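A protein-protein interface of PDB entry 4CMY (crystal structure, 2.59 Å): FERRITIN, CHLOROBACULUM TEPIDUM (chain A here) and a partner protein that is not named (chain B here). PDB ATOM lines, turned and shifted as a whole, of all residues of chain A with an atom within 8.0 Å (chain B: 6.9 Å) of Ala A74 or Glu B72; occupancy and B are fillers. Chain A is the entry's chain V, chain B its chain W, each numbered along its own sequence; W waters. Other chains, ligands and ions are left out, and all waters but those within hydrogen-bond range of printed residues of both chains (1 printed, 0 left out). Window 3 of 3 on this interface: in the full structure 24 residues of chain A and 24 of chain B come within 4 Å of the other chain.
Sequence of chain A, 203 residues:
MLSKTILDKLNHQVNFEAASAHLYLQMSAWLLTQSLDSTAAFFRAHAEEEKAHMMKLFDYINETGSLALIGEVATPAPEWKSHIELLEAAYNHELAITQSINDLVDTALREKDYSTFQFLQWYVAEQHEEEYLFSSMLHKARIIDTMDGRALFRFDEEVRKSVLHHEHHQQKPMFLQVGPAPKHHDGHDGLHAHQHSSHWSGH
Ala A74 touches just one residue of chain B: Glu B72 (3.9 Å).
Printed residues of chain A within 4 Å of Glu B72: Val A73 (3.5 Å) and Ala A74 (3.9 Å).
Gly B71 touches just one residue of chain A: Thr A75 (3.4 Å).
Printed residues of chain B within 4 Å of Val A73: Glu B72 (3.5 Å) and Val B73 (2.9 Å).
Printed residues of chain B within 4 Å of Glu A72: Val B73 (3.6 Å) and Ala B74 (3.9 Å).
Of the printed residues of chain A, Ile B70 touches His A22.
Ala A77 touches none of the printed residues of chain B.
Pro A76 touches none of the printed residues of chain B.
The nearest residue of chain B that does not touch Ala A74 is Gly B71 (4.4 Å).
His A22 touches Ile B70 (ND1 to CG2, 3.5 Å).
His A22 touches Val B73.
Glu A72 touches Val B73.
Glu A72 touches Ala B74.
Glu B72 touches Val A73.
Ala A74 touches Glu B72.
Water W1 lies within hydrogen-bond range of OG1 of Thr A75, O of Gly B71, ND1 of His A22 and O of Val A73.
O of Glu A72 lies close to OD1 of Asn A15.
OD1 of Asn B15 lies close to O of Ile B70 (2.9 Å).
OD1 of Asn B15 lies close to O of Glu B72 (2.8 Å).
Of the 13 printed residues of chain A, 5 touch a printed residue of chain B.
Printed residues of chain A that touch a printed residue of chain B: His A22, Glu A72, Val A73, Ala A74 and Thr A75.
Hydrophobic or aromatic side chains of chain A within 4 Å of the printed part of chain B: His A22 and Ala A74.
Of the 7 printed residues of chain B, 5 touch a printed residue of chain A.
Printed residues of chain B that touch a printed residue of chain A: Ile B70, Gly B71, Glu B72, Val B73 and Ala B74.
Among the printed residues, 8 pairs touch across the chains.
The backbone NH of Val B73 is in hydrogen-bond range of the backbone carbonyl oxygen of Val A73, at 2.9 Å.
The backbone NH (N) of Thr A75 lies within hydrogen-bond range of the backbone carbonyl oxygen (O) of Gly B71, 3.4 Å away.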
ATOM      1  N   ASN A  15       2.614 -11.833  16.989  1.00  0.00           N
ATOM      2  CA  ASN A  15       3.659 -12.726  16.530  1.00  0.00           C
ATOM      3  C   ASN A  15       3.798 -12.715  15.014  1.00  0.00           C
ATOM      4  O   ASN A  15       4.889 -12.790  14.464  1.00  0.00           O
ATOM      5  CB  ASN A  15       3.342 -14.136  17.053  1.00  0.00           C
ATOM      6  CG  ASN A  15       4.300 -15.167  16.563  1.00  0.00           C
ATOM      7  OD1 ASN A  15       5.279 -15.478  17.224  1.00  0.00           O
ATOM      8  ND2 ASN A  15       4.048 -15.685  15.370  1.00  0.00           N
ATOM      9  N   ALA A  18       5.606  -9.555  13.983  1.00  0.00           N
ATOM     10  CA  ALA A  18       7.019  -9.767  14.276  1.00  0.00           C
ATOM     11  C   ALA A  18       7.696 -10.624  13.204  1.00  0.00           C
ATOM     12  O   ALA A  18       8.802 -10.332  12.789  1.00  0.00           O
ATOM     13  CB  ALA A  18       7.188 -10.421  15.623  1.00  0.00           C
ATOM     14  N   ALA A  19       7.029 -11.692  12.785  1.00  0.00           N
ATOM     15  CA  ALA A  19       7.576 -12.564  11.761  1.00  0.00           C
ATOM     16  C   ALA A  19       7.703 -11.851  10.453  1.00  0.00           C
ATOM     17  O   ALA A  19       8.599 -12.150   9.674  1.00  0.00           O
ATOM     18  CB  ALA A  19       6.712 -13.794  11.600  1.00  0.00           C
ATOM     19  N   SER A  20       6.806 -10.901  10.181  1.00  0.00           N
ATOM     20  CA  SER A  20       6.874 -10.125   8.930  1.00  0.00           C
ATOM     21  C   SER A  20       8.078  -9.226   8.905  1.00  0.00           C
ATOM     22  O   SER A  20       8.749  -9.127   7.908  1.00  0.00           O
ATOM     23  CB  SER A  20       5.624  -9.278   8.752  1.00  0.00           C
ATOM     24  OG  SER A  20       4.474 -10.095   8.849  1.00  0.00           O
ATOM     25  N   HIS A  22      10.881  -9.749  10.415  1.00  0.00           N
ATOM     26  CA  HIS A  22      12.062 -10.622  10.232  1.00  0.00           C
ATOM     27  C   HIS A  22      12.130 -11.135   8.804  1.00  0.00           C
ATOM     28  O   HIS A  22      13.185 -11.191   8.234  1.00  0.00           O
ATOM     29  CB  HIS A  22      12.008 -11.782  11.221  1.00  0.00           C
ATOM     30  CG  HIS A  22      12.411 -11.385  12.595  1.00  0.00           C
ATOM     31  ND1 HIS A  22      12.781 -12.273  13.573  1.00  0.00           N
ATOM     32  CD2 HIS A  22      12.520 -10.159  13.145  1.00  0.00           C
ATOM     33  CE1 HIS A  22      13.072 -11.612  14.682  1.00  0.00           C
ATOM     34  NE2 HIS A  22      12.904 -10.327  14.451  1.00  0.00           N
ATOM     35  N   LEU A  23      10.983 -11.469   8.234  1.00  0.00           N
ATOM     36  CA  LEU A  23      10.919 -11.906   6.851  1.00  0.00           C
ATOM     37  C   LEU A  23      11.471 -10.831   5.932  1.00  0.00           C
ATOM     38  O   LEU A  23      12.265 -11.105   5.061  1.00  0.00           O
ATOM     39  CB  LEU A  23       9.487 -12.282   6.464  1.00  0.00           C
ATOM     40  CG  LEU A  23       9.289 -12.766   5.022  1.00  0.00           C
ATOM     41  CD1 LEU A  23      10.075 -14.031   4.750  1.00  0.00           C
ATOM     42  CD2 LEU A  23       7.814 -13.026   4.715  1.00  0.00           C
ATOM     43  N   GLY A  71       5.993 -14.772  21.572  1.00  0.00           N
ATOM     44  CA  GLY A  71       6.066 -16.126  21.044  1.00  0.00           C
ATOM     45  C   GLY A  71       7.332 -16.464  20.273  1.00  0.00           C
ATOM     46  O   GLY A  71       8.344 -15.770  20.382  1.00  0.00           O
ATOM     47  N   GLU A  72       7.252 -17.521  19.456  1.00  0.00           N
ATOM     48  CA  GLU A  72       8.366 -17.967  18.619  1.00  0.00           C
ATOM     49  C   GLU A  72       8.225 -17.384  17.250  1.00  0.00           C
ATOM     50  O   GLU A  72       7.161 -17.430  16.659  1.00  0.00           O
ATOM     51  CB  GLU A  72       8.358 -19.480  18.459  1.00  0.00           C
ATOM     52  CG  GLU A  72       8.456 -20.252  19.773  1.00  0.00           C
ATOM     53  CD  GLU A  72       8.528 -21.774  19.579  1.00  0.00           C
ATOM     54  OE1 GLU A  72       8.928 -22.230  18.474  1.00  0.00           O
ATOM     55  OE2 GLU A  72       8.192 -22.504  20.555  1.00  0.00           O
ATOM     56  N   VAL A  73       9.319 -16.892  16.708  1.00  0.00           N
ATOM     57  CA  VAL A  73       9.327 -16.363  15.361  1.00  0.00           C
ATOM     58  C   VAL A  73      10.398 -17.089  14.587  1.00  0.00           C
ATOM     59  O   VAL A  73      11.579 -17.034  14.985  1.00  0.00           O
ATOM     60  CB  VAL A  73       9.659 -14.865  15.412  1.00  0.00           C
ATOM     61  CG1 VAL A  73       9.688 -14.286  14.013  1.00  0.00           C
ATOM     62  CG2 VAL A  73       8.647 -14.123  16.246  1.00  0.00           C
ATOM     63  N   ALA A  74      10.045 -17.783  13.511  1.00  0.00           N
ATOM     64  CA  ALA A  74      11.072 -18.565  12.778  1.00  0.00           C
ATOM     65  C   ALA A  74      11.159 -18.066  11.385  1.00  0.00           C
ATOM     66  O   ALA A  74      10.172 -18.053  10.699  1.00  0.00           O
ATOM     67  CB  ALA A  74      10.773 -20.080  12.784  1.00  0.00           C
ATOM     68  N   THR A  75      12.343 -17.668  10.955  1.00  0.00           N
ATOM     69  CA  THR A  75      12.493 -17.123   9.621  1.00  0.00           C
ATOM     70  C   THR A  75      13.288 -18.089   8.837  1.00  0.00           C
ATOM     71  O   THR A  75      14.487 -18.285   9.126  1.00  0.00           O
ATOM     72  CB  THR A  75      13.199 -15.744   9.626  1.00  0.00           C
ATOM     73  OG1 THR A  75      12.522 -14.877  10.545  1.00  0.00           O
ATOM     74  CG2 THR A  75      13.186 -15.116   8.226  1.00  0.00           C
ATOM     75  N   PRO A  76      12.664 -18.666   7.806  1.00  0.00           N
ATOM     76  CA  PRO A  76      13.448 -19.568   6.951  1.00  0.00           C
ATOM     77  C   PRO A  76      14.556 -18.829   6.189  1.00  0.00           C
ATOM     78  O   PRO A  76      14.418 -17.641   5.868  1.00  0.00           O
ATOM     79  CB  PRO A  76      12.406 -20.142   5.977  1.00  0.00           C
ATOM     80  CG  PRO A  76      11.361 -19.082   5.890  1.00  0.00           C
ATOM     81  CD  PRO A  76      11.337 -18.388   7.236  1.00  0.00           C
ATOM     82  N   ALA A  77      15.673 -19.530   5.974  1.00  0.00           N
ATOM     83  CA  ALA A  77      16.751 -18.999   5.167  1.00  0.00           C
ATOM     84  C   ALA A  77      16.169 -18.630   3.786  1.00  0.00           C
ATOM     85  O   ALA A  77      15.159 -19.151   3.376  1.00  0.00           O
ATOM     86  CB  ALA A  77      17.907 -20.007   5.081  1.00  0.00           C
ATOM     87  N   ASN B  15      21.260 -13.070  15.734  1.00  0.00           N
ATOM     88  CA  ASN B  15      20.116 -13.741  16.293  1.00  0.00           C
ATOM     89  C   ASN B  15      19.990 -13.502  17.791  1.00  0.00           C
ATOM     90  O   ASN B  15      18.905 -13.372  18.322  1.00  0.00           O
ATOM     91  CB  ASN B  15      20.247 -15.230  15.957  1.00  0.00           C
ATOM     92  CG  ASN B  15      19.156 -16.054  16.584  1.00  0.00           C
ATOM     93  OD1 ASN B  15      18.138 -16.332  15.967  1.00  0.00           O
ATOM     94  ND2 ASN B  15      19.364 -16.445  17.818  1.00  0.00           N
ATOM     95  N   ALA B  19      16.927 -11.825  19.803  1.00  0.00           N
ATOM     96  CA  ALA B  19      16.303 -12.466  20.949  1.00  0.00           C
ATOM     97  C   ALA B  19      16.299 -11.576  22.188  1.00  0.00           C
ATOM     98  O   ALA B  19      15.351 -11.618  22.963  1.00  0.00           O
ATOM     99  CB  ALA B  19      16.996 -13.762  21.289  1.00  0.00           C
ATOM    100  N   ILE B  70      18.748 -14.140  10.085  1.00  0.00           N
ATOM    101  CA  ILE B  70      18.054 -13.807  11.311  1.00  0.00           C
ATOM    102  C   ILE B  70      17.832 -15.049  12.198  1.00  0.00           C
ATOM    103  O   ILE B  70      18.051 -14.994  13.417  1.00  0.00           O
ATOM    104  CB  ILE B  70      16.666 -13.211  11.048  1.00  0.00           C
ATOM    105  CG1 ILE B  70      16.729 -12.087  10.032  1.00  0.00           C
ATOM    106  CG2 ILE B  70      16.080 -12.691  12.371  1.00  0.00           C
ATOM    107  CD1 ILE B  70      17.427 -10.843  10.523  1.00  0.00           C
ATOM    108  N   GLY B  71      17.422 -16.153  11.588  1.00  0.00           N
ATOM    109  CA  GLY B  71      17.224 -17.399  12.307  1.00  0.00           C
ATOM    110  C   GLY B  71      15.931 -17.453  13.103  1.00  0.00           C
ATOM    111  O   GLY B  71      15.031 -16.683  12.862  1.00  0.00           O
ATOM    112  N   GLU B  72      15.865 -18.386  14.053  1.00  0.00           N
ATOM    113  CA  GLU B  72      14.700 -18.578  14.915  1.00  0.00           C
ATOM    114  C   GLU B  72      14.930 -17.839  16.201  1.00  0.00           C
ATOM    115  O   GLU B  72      16.012 -17.932  16.790  1.00  0.00           O
ATOM    116  CB  GLU B  72      14.525 -20.040  15.282  1.00  0.00           C
ATOM    117  CG  GLU B  72      14.328 -20.966  14.090  1.00  0.00           C
ATOM    118  CD  GLU B  72      14.064 -22.424  14.491  1.00  0.00           C
ATOM    119  OE1 GLU B  72      13.596 -22.662  15.640  1.00  0.00           O
ATOM    120  OE2 GLU B  72      14.319 -23.325  13.634  1.00  0.00           O
ATOM    121  N   VAL B  73      13.907 -17.153  16.677  1.00  0.00           N
ATOM    122  CA  VAL B  73      13.987 -16.424  17.924  1.00  0.00           C
ATOM    123  C   VAL B  73      12.828 -16.882  18.769  1.00  0.00           C
ATOM    124  O   VAL B  73      11.690 -16.736  18.362  1.00  0.00           O
ATOM    125  CB  VAL B  73      13.853 -14.927  17.658  1.00  0.00           C
ATOM    126  CG1 VAL B  73      13.933 -14.169  18.951  1.00  0.00           C
ATOM    127  CG2 VAL B  73      14.953 -14.443  16.719  1.00  0.00           C
ATOM    128  N   ALA B  74      13.095 -17.482  19.920  1.00  0.00           N
ATOM    129  CA  ALA B  74      11.996 -18.003  20.741  1.00  0.00           C
ATOM    130  C   ALA B  74      12.008 -17.309  22.075  1.00  0.00           C
ATOM    131  O   ALA B  74      12.987 -17.375  22.768  1.00  0.00           O
ATOM    132  CB  ALA B  74      12.097 -19.531  20.936  1.00  0.00           C
HETATM  133  O   HOH W   1      12.858 -15.056  13.176  1.00  0.00           O
